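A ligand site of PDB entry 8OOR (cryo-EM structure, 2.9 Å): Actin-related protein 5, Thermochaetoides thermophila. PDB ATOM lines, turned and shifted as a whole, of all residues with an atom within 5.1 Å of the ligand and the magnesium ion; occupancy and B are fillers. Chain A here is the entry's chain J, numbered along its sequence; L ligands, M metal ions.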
ATOM      1  N   ASP A  62     -38.260   2.690   0.573  1.00  0.00           N
ATOM      2  CA  ASP A  62     -37.284   3.261   1.491  1.00  0.00           C
ATOM      3  C   ASP A  62     -37.369   4.775   1.390  1.00  0.00           C
ATOM      4  O   ASP A  62     -36.901   5.370   0.422  1.00  0.00           O
ATOM      5  CB  ASP A  62     -35.894   2.720   1.204  1.00  0.00           C
ATOM      6  CG  ASP A  62     -34.851   3.285   2.130  1.00  0.00           C
ATOM      7  OD1 ASP A  62     -35.187   3.572   3.293  1.00  0.00           O
ATOM      8  OD2 ASP A  62     -33.690   3.401   1.711  1.00  0.00           O
ATOM      9  N   ASN A  63     -37.977   5.389   2.402  1.00  0.00           N
ATOM     10  CA  ASN A  63     -38.349   6.805   2.378  1.00  0.00           C
ATOM     11  C   ASN A  63     -37.176   7.719   2.744  1.00  0.00           C
ATOM     12  O   ASN A  63     -37.203   8.436   3.742  1.00  0.00           O
ATOM     13  CB  ASN A  63     -39.539   6.989   3.310  1.00  0.00           C
ATOM     14  CG  ASN A  63     -40.165   8.344   3.206  1.00  0.00           C
ATOM     15  OD1 ASN A  63     -40.164   8.966   2.152  1.00  0.00           O
ATOM     16  ND2 ASN A  63     -40.721   8.811   4.320  1.00  0.00           N
ATOM     17  N   GLY A  64     -36.114   7.636   1.951  1.00  0.00           N
ATOM     18  CA  GLY A  64     -34.870   8.334   2.279  1.00  0.00           C
ATOM     19  C   GLY A  64     -34.882   9.828   1.945  1.00  0.00           C
ATOM     20  O   GLY A  64     -35.172  10.212   0.817  1.00  0.00           O
ATOM     21  N   SER A  65     -34.471  10.649   2.918  1.00  0.00           N
ATOM     22  CA  SER A  65     -34.381  12.095   2.717  1.00  0.00           C
ATOM     23  C   SER A  65     -33.415  12.482   1.610  1.00  0.00           C
ATOM     24  O   SER A  65     -33.563  13.535   0.994  1.00  0.00           O
ATOM     25  CB  SER A  65     -33.946  12.778   3.996  1.00  0.00           C
ATOM     26  OG  SER A  65     -34.685  12.307   5.095  1.00  0.00           O
ATOM     27  N   HIS A  66     -32.410  11.660   1.359  1.00  0.00           N
ATOM     28  CA  HIS A  66     -31.559  11.866   0.195  1.00  0.00           C
ATOM     29  C   HIS A  66     -32.168  11.258  -1.054  1.00  0.00           C
ATOM     30  O   HIS A  66     -32.107  11.866  -2.123  1.00  0.00           O
ATOM     31  CB  HIS A  66     -30.187  11.272   0.462  1.00  0.00           C
ATOM     32  CG  HIS A  66     -29.231  11.417  -0.669  1.00  0.00           C
ATOM     33  ND1 HIS A  66     -28.814  12.642  -1.140  1.00  0.00           N
ATOM     34  CD2 HIS A  66     -28.665  10.488  -1.467  1.00  0.00           C
ATOM     35  CE1 HIS A  66     -27.994  12.456  -2.154  1.00  0.00           C
ATOM     36  NE2 HIS A  66     -27.882  11.159  -2.376  1.00  0.00           N
ATOM     37  N   SER A  67     -32.727  10.057  -0.948  1.00  0.00           N
ATOM     38  CA  SER A  67     -33.230   9.336  -2.103  1.00  0.00           C
ATOM     39  C   SER A  67     -34.362   8.427  -1.669  1.00  0.00           C
ATOM     40  O   SER A  67     -34.170   7.589  -0.788  1.00  0.00           O
ATOM     41  CB  SER A  67     -32.119   8.538  -2.758  1.00  0.00           C
ATOM     42  OG  SER A  67     -32.589   7.884  -3.922  1.00  0.00           O
ATOM     43  N   ARG A  69     -36.244   5.270  -2.494  1.00  0.00           N
ATOM     44  CA  ARG A  69     -36.000   4.025  -3.201  1.00  0.00           C
ATOM     45  C   ARG A  69     -37.234   3.148  -3.131  1.00  0.00           C
ATOM     46  O   ARG A  69     -37.758   2.896  -2.040  1.00  0.00           O
ATOM     47  CB  ARG A  69     -34.803   3.324  -2.574  1.00  0.00           C
ATOM     48  CG  ARG A  69     -33.520   4.037  -2.832  1.00  0.00           C
ATOM     49  CD  ARG A  69     -32.510   3.628  -1.838  1.00  0.00           C
ATOM     50  NE  ARG A  69     -32.848   4.249  -0.571  1.00  0.00           N
ATOM     51  CZ  ARG A  69     -32.138   5.206   0.017  1.00  0.00           C
ATOM     52  NH1 ARG A  69     -31.031   5.665  -0.519  1.00  0.00           N
ATOM     53  NH2 ARG A  69     -32.559   5.713   1.161  1.00  0.00           N
ATOM     54  N   GLY A 124     -34.861  14.177   9.490  1.00  0.00           N
ATOM     55  CA  GLY A 124     -35.279  12.934   8.898  1.00  0.00           C
ATOM     56  C   GLY A 124     -36.770  12.759   8.803  1.00  0.00           C
ATOM     57  O   GLY A 124     -37.244  11.677   8.465  1.00  0.00           O
ATOM     58  N   ASP A 190     -34.792   1.970   8.729  1.00  0.00           N
ATOM     59  CA  ASP A 190     -33.814   1.625   7.691  1.00  0.00           C
ATOM     60  C   ASP A 190     -32.502   1.098   8.286  1.00  0.00           C
ATOM     61  O   ASP A 190     -31.860   0.231   7.678  1.00  0.00           O
ATOM     62  CB  ASP A 190     -33.554   2.833   6.789  1.00  0.00           C
ATOM     63  CG  ASP A 190     -32.784   3.965   7.477  1.00  0.00           C
ATOM     64  OD1 ASP A 190     -32.687   3.992   8.724  1.00  0.00           O
ATOM     65  OD2 ASP A 190     -32.264   4.843   6.741  1.00  0.00           O
ATOM     66  N   SER A 209     -26.578   8.882   8.039  1.00  0.00           N
ATOM     67  CA  SER A 209     -27.477   9.027   6.921  1.00  0.00           C
ATOM     68  C   SER A 209     -27.343  10.438   6.369  1.00  0.00           C
ATOM     69  O   SER A 209     -26.378  11.149   6.653  1.00  0.00           O
ATOM     70  CB  SER A 209     -28.914   8.750   7.372  1.00  0.00           C
ATOM     71  OG  SER A 209     -29.009   7.537   8.079  1.00  0.00           O
ATOM     72  N   TYR A 210     -28.303  10.831   5.550  1.00  0.00           N
ATOM     73  CA  TYR A 210     -28.420  12.227   5.160  1.00  0.00           C
ATOM     74  C   TYR A 210     -28.752  13.089   6.376  1.00  0.00           C
ATOM     75  O   TYR A 210     -28.154  14.142   6.602  1.00  0.00           O
ATOM     76  CB  TYR A 210     -29.488  12.360   4.087  1.00  0.00           C
ATOM     77  CG  TYR A 210     -29.340  13.548   3.168  1.00  0.00           C
ATOM     78  CD1 TYR A 210     -28.227  13.666   2.359  1.00  0.00           C
ATOM     79  CD2 TYR A 210     -30.308  14.524   3.091  1.00  0.00           C
ATOM     80  CE1 TYR A 210     -28.076  14.732   1.514  1.00  0.00           C
ATOM     81  CE2 TYR A 210     -30.177  15.577   2.239  1.00  0.00           C
ATOM     82  CZ  TYR A 210     -29.055  15.683   1.464  1.00  0.00           C
ATOM     83  OH  TYR A 210     -28.910  16.740   0.597  1.00  0.00           O
ATOM     84  N   SER A 211     -29.739  12.667   7.154  1.00  0.00           N
ATOM     85  CA  SER A 211     -30.350  13.521   8.162  1.00  0.00           C
ATOM     86  C   SER A 211     -29.664  13.493   9.524  1.00  0.00           C
ATOM     87  O   SER A 211     -29.770  14.466  10.261  1.00  0.00           O
ATOM     88  CB  SER A 211     -31.803  13.123   8.339  1.00  0.00           C
ATOM     89  OG  SER A 211     -31.908  11.806   8.841  1.00  0.00           O
ATOM     90  N   ALA A 212     -29.036  12.387   9.904  1.00  0.00           N
ATOM     91  CA  ALA A 212     -28.621  12.214  11.291  1.00  0.00           C
ATOM     92  C   ALA A 212     -27.638  11.068  11.372  1.00  0.00           C
ATOM     93  O   ALA A 212     -27.435  10.321  10.411  1.00  0.00           O
ATOM     94  CB  ALA A 212     -29.807  11.949  12.222  1.00  0.00           C
ATOM     95  N   GLY A 235     -25.087  13.536   6.338  1.00  0.00           N
ATOM     96  CA  GLY A 235     -24.543  13.894   5.046  1.00  0.00           C
ATOM     97  C   GLY A 235     -25.073  15.191   4.479  1.00  0.00           C
ATOM     98  O   GLY A 235     -24.407  15.798   3.626  1.00  0.00           O
ATOM     99  N   TRP A 236     -26.266  15.598   4.876  1.00  0.00           N
ATOM    100  CA  TRP A 236     -26.781  16.913   4.528  1.00  0.00           C
ATOM    101  C   TRP A 236     -26.004  18.017   5.217  1.00  0.00           C
ATOM    102  O   TRP A 236     -25.639  19.018   4.599  1.00  0.00           O
ATOM    103  CB  TRP A 236     -28.253  17.028   4.893  1.00  0.00           C
ATOM    104  CG  TRP A 236     -28.836  18.349   4.579  1.00  0.00           C
ATOM    105  CD1 TRP A 236     -29.351  18.738   3.386  1.00  0.00           C
ATOM    106  CD2 TRP A 236     -28.978  19.459   5.456  1.00  0.00           C
ATOM    107  NE1 TRP A 236     -29.808  20.017   3.475  1.00  0.00           N
ATOM    108  CE2 TRP A 236     -29.583  20.483   4.737  1.00  0.00           C
ATOM    109  CE3 TRP A 236     -28.630  19.685   6.785  1.00  0.00           C
ATOM    110  CZ2 TRP A 236     -29.861  21.712   5.292  1.00  0.00           C
ATOM    111  CZ3 TRP A 236     -28.911  20.907   7.334  1.00  0.00           C
ATOM    112  CH2 TRP A 236     -29.526  21.906   6.600  1.00  0.00           C
ATOM    113  N   GLU A 264     -21.943  18.804  -1.854  1.00  0.00           N
ATOM    114  CA  GLU A 264     -22.259  17.413  -1.579  1.00  0.00           C
ATOM    115  C   GLU A 264     -21.428  16.438  -2.412  1.00  0.00           C
ATOM    116  O   GLU A 264     -20.972  15.415  -1.897  1.00  0.00           O
ATOM    117  CB  GLU A 264     -23.749  17.194  -1.784  1.00  0.00           C
ATOM    118  CG  GLU A 264     -24.234  15.895  -1.270  1.00  0.00           C
ATOM    119  CD  GLU A 264     -25.640  15.638  -1.684  1.00  0.00           C
ATOM    120  OE1 GLU A 264     -26.553  16.112  -0.994  1.00  0.00           O
ATOM    121  OE2 GLU A 264     -25.831  14.985  -2.727  1.00  0.00           O
ATOM    122  N   VAL A 267     -17.855  16.643  -0.969  1.00  0.00           N
ATOM    123  CA  VAL A 267     -17.717  15.837   0.253  1.00  0.00           C
ATOM    124  C   VAL A 267     -17.641  14.356  -0.091  1.00  0.00           C
ATOM    125  O   VAL A 267     -16.843  13.618   0.488  1.00  0.00           O
ATOM    126  CB  VAL A 267     -18.881  16.122   1.205  1.00  0.00           C
ATOM    127  CG1 VAL A 267     -18.931  15.081   2.285  1.00  0.00           C
ATOM    128  CG2 VAL A 267     -18.714  17.494   1.808  1.00  0.00           C
ATOM    129  N   ARG A 268     -18.487  13.911  -0.994  1.00  0.00           N
ATOM    130  CA  ARG A 268     -18.421  12.529  -1.451  1.00  0.00           C
ATOM    131  C   ARG A 268     -17.082  12.200  -2.084  1.00  0.00           C
ATOM    132  O   ARG A 268     -16.458  11.180  -1.760  1.00  0.00           O
ATOM    133  CB  ARG A 268     -19.571  12.266  -2.414  1.00  0.00           C
ATOM    134  CG  ARG A 268     -19.756  10.824  -2.736  1.00  0.00           C
ATOM    135  CD  ARG A 268     -20.949  10.631  -3.625  1.00  0.00           C
ATOM    136  NE  ARG A 268     -22.137  11.178  -2.977  1.00  0.00           N
ATOM    137  CZ  ARG A 268     -23.064  11.899  -3.587  1.00  0.00           C
ATOM    138  NH1 ARG A 268     -23.105  12.016  -4.901  1.00  0.00           N
ATOM    139  NH2 ARG A 268     -24.023  12.450  -2.853  1.00  0.00           N
ATOM    140  N   GLY A 690     -25.627   3.134   6.294  1.00  0.00           N
ATOM    141  CA  GLY A 690     -25.954   4.428   5.743  1.00  0.00           C
ATOM    142  C   GLY A 690     -24.842   5.055   4.936  1.00  0.00           C
ATOM    143  O   GLY A 690     -23.663   4.850   5.218  1.00  0.00           O
ATOM    144  N   GLY A 691     -25.222   5.775   3.884  1.00  0.00           N
ATOM    145  CA  GLY A 691     -24.257   6.264   2.914  1.00  0.00           C
ATOM    146  C   GLY A 691     -23.180   7.148   3.506  1.00  0.00           C
ATOM    147  O   GLY A 691     -22.020   7.090   3.088  1.00  0.00           O
ATOM    148  N   ASN A 692     -23.530   7.962   4.492  1.00  0.00           N
ATOM    149  CA  ASN A 692     -22.587   8.902   5.079  1.00  0.00           C
ATOM    150  C   ASN A 692     -21.512   8.231   5.934  1.00  0.00           C
ATOM    151  O   ASN A 692     -20.692   8.938   6.514  1.00  0.00           O
ATOM    152  CB  ASN A 692     -23.377   9.966   5.843  1.00  0.00           C
ATOM    153  CG  ASN A 692     -22.518  11.090   6.389  1.00  0.00           C
ATOM    154  OD1 ASN A 692     -22.482  11.335   7.584  1.00  0.00           O
ATOM    155  ND2 ASN A 692     -21.809  11.758   5.492  1.00  0.00           N
ATOM    156  N   LEU A 694     -19.560   6.039   4.316  1.00  0.00           N
ATOM    157  CA  LEU A 694     -18.667   5.507   3.293  1.00  0.00           C
ATOM    158  C   LEU A 694     -17.320   6.221   3.212  1.00  0.00           C
ATOM    159  O   LEU A 694     -16.536   5.853   2.334  1.00  0.00           O
ATOM    160  CB  LEU A 694     -19.374   5.559   1.944  1.00  0.00           C
ATOM    161  CG  LEU A 694     -20.443   4.496   1.732  1.00  0.00           C
ATOM    162  CD1 LEU A 694     -21.198   4.769   0.459  1.00  0.00           C
ATOM    163  CD2 LEU A 694     -19.787   3.155   1.656  1.00  0.00           C
ATOM    164  N   PHE A 695     -17.043   7.207   4.047  1.00  0.00           N
ATOM    165  CA  PHE A 695     -15.731   7.840   4.058  1.00  0.00           C
ATOM    166  C   PHE A 695     -14.626   6.818   4.302  1.00  0.00           C
ATOM    167  O   PHE A 695     -14.796   5.864   5.039  1.00  0.00           O
ATOM    168  CB  PHE A 695     -15.671   8.898   5.152  1.00  0.00           C
ATOM    169  CG  PHE A 695     -16.668   9.982   4.999  1.00  0.00           C
ATOM    170  CD1 PHE A 695     -16.609  10.851   3.932  1.00  0.00           C
ATOM    171  CD2 PHE A 695     -17.679  10.129   5.916  1.00  0.00           C
ATOM    172  CE1 PHE A 695     -17.531  11.837   3.789  1.00  0.00           C
ATOM    173  CE2 PHE A 695     -18.600  11.115   5.774  1.00  0.00           C
ATOM    174  CZ  PHE A 695     -18.529  11.972   4.716  1.00  0.00           C
ATOM    175  N   ALA A 724     -23.938   0.352   1.531  1.00  0.00           N
ATOM    176  CA  ALA A 724     -24.350   1.289   2.557  1.00  0.00           C
ATOM    177  C   ALA A 724     -25.685   1.972   2.304  1.00  0.00           C
ATOM    178  O   ALA A 724     -26.217   2.590   3.221  1.00  0.00           O
ATOM    179  CB  ALA A 724     -23.266   2.356   2.755  1.00  0.00           C
ATOM    180  N   ILE A 725     -26.254   1.868   1.098  1.00  0.00           N
ATOM    181  CA  ILE A 725     -27.405   2.676   0.729  1.00  0.00           C
ATOM    182  C   ILE A 725     -28.590   1.816   0.264  1.00  0.00           C
ATOM    183  O   ILE A 725     -29.724   2.027   0.701  1.00  0.00           O
ATOM    184  CB  ILE A 725     -27.035   3.735  -0.342  1.00  0.00           C
ATOM    185  CG1 ILE A 725     -26.568   3.078  -1.633  1.00  0.00           C
ATOM    186  CG2 ILE A 725     -25.975   4.673   0.175  1.00  0.00           C
ATOM    187  CD1 ILE A 725     -26.232   4.056  -2.713  1.00  0.00           C
HETATM  188  P1  LIG L   1     -32.213   9.251   5.923  1.00  0.00           P
HETATM  189  O1  LIG L   1     -32.425   7.981   6.673  1.00  0.00           O
HETATM  190  O2  LIG L   1     -33.449   9.731   5.235  1.00  0.00           O
HETATM  191  O3  LIG L   1     -31.619  10.348   6.756  1.00  0.00           O
HETATM  192  P2  LIG L   1     -31.094   8.303   3.454  1.00  0.00           P
HETATM  193  O4  LIG L   1     -31.571   6.917   3.584  1.00  0.00           O
HETATM  194  O5  LIG L   1     -31.649   9.192   2.381  1.00  0.00           O
HETATM  195  O6  LIG L   1     -31.205   9.030   4.787  1.00  0.00           O
HETATM  196  P3  LIG L   1     -28.497   7.495   2.417  1.00  0.00           P
HETATM  197  O7  LIG L   1     -28.157   6.219   3.071  1.00  0.00           O
HETATM  198  O8  LIG L   1     -28.986   7.489   0.985  1.00  0.00           O
HETATM  199  O9  LIG L   1     -29.519   8.272   3.269  1.00  0.00           O
HETATM  200  O10 LIG L   1     -27.265   8.466   2.496  1.00  0.00           O
HETATM  201  C1  LIG L   1     -26.908   9.325   1.394  1.00  0.00           C
HETATM  202  C2  LIG L   1     -25.845  10.243   1.923  1.00  0.00           C
HETATM  203  O11 LIG L   1     -24.566   9.588   1.827  1.00  0.00           O
HETATM  204  C3  LIG L   1     -25.694  11.563   1.168  1.00  0.00           C
HETATM  205  O12 LIG L   1     -25.259  12.579   2.053  1.00  0.00           O
HETATM  206  C4  LIG L   1     -24.604  11.231   0.158  1.00  0.00           C
HETATM  207  O13 LIG L   1     -23.886  12.376  -0.275  1.00  0.00           O
HETATM  208  C5  LIG L   1     -23.700  10.345   1.007  1.00  0.00           C
HETATM  209  N1  LIG L   1     -22.852   9.447   0.239  1.00  0.00           N
HETATM  210  C6  LIG L   1     -23.219   8.673  -0.836  1.00  0.00           C
HETATM  211  N2  LIG L   1     -22.233   7.991  -1.359  1.00  0.00           N
HETATM  212  C7  LIG L   1     -21.142   8.341  -0.578  1.00  0.00           C
HETATM  213  C8  LIG L   1     -19.791   7.959  -0.597  1.00  0.00           C
HETATM  214  N3  LIG L   1     -19.285   7.095  -1.482  1.00  0.00           N
HETATM  215  N4  LIG L   1     -18.962   8.487   0.323  1.00  0.00           N
HETATM  216  C9  LIG L   1     -19.468   9.351   1.209  1.00  0.00           C
HETATM  217  N5  LIG L   1     -20.723   9.778   1.333  1.00  0.00           N
HETATM  218  C10 LIG L   1     -21.512   9.238   0.408  1.00  0.00           C
HETATM  219 MG    MG M   1     -31.955   6.402   5.384  1.00  0.00          MG
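O3 of the ligand sits at hydrogen-bond distance from N of Ser 211, 3.0 Å away. OG of Ser 211 lies within hydrogen-bond range of O3 of the ligand (2.6 Å). NH2 of Arg 268 is in hydrogen-bond range of O13 of the ligand. The backbone NH of Ser 65 sits at hydrogen-bond distance from an oxygen (O2) of the ligand. OG of Ser 65 is in hydrogen-bond range of O2 of the ligand (2.9 Å). O5 of the ligand is in hydrogen-bond range of N of His 66, at 2.8 Å. O8 of the ligand is in salt-bridge range of NH1 of Arg 69. The backbone NH (N) of Gly 691 is in hydrogen-bond range of an oxygen (O7) of the ligand (3.1 Å). N of Tyr 210 lies within hydrogen-bond range of O6 of the ligand (3.5 Å). An oxygen (O11) of the ligand is in hydrogen-bond range of the backbone NH of Asn 692 (3.3 Å).
NH2 of Arg 69 lies within hydrogen-bond range of O of Ser 67. The guanidinium group (NE) of Arg 69 lies within salt-bridge range of the side-chain carboxylate (OD2) of Asp 62. The backbone NH (N) of Gly 691 is in hydrogen-bond range of the backbone carbonyl oxygen (O) of Ala 724 (3.4 Å). The backbone carbonyl oxygen (O) of Tyr 210 is in hydrogen-bond range of the backbone NH (N) of Gly 235. OE1 of Glu 264 lies within hydrogen-bond range of OH of Tyr 210 (2.9 Å). O of Tyr 210 is in hydrogen-bond range of N of Trp 236 (2.9 Å). The backbone carbonyl oxygen (O) of Ser 209 sits at hydrogen-bond distance from the backbone NH (N) of Gly 235 (2.7 Å). The backbone NH of Gly 690 sits close to the backbone carbonyl oxygen of Ala 724, 3.2 Å away.
Merely in contact with the ligand: Gly 64 (3.3 Å), Ser 67 (3.6 Å), Ser 209 (3.2 Å), Gly 235 (3.3 Å), Glu 264 (3.7 Å), Gly 690 (3.9 Å), Leu 694 (3.4 Å) and Ile 725 (3.9 Å). Hydrophobic or aromatic side chains that line the ligand: His 66, Tyr 210, Leu 694 and Ile 725.
The magnesium ion is bound by O4 of the ligand (1.9 Å), OD2 of Asp 190 (2.1 Å) and O1 of the ligand (2.1 Å). The magnesium ion has three donor atoms within binding distance. Slightly farther from the magnesium ion lies O6 of the ligand (2.8 Å).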
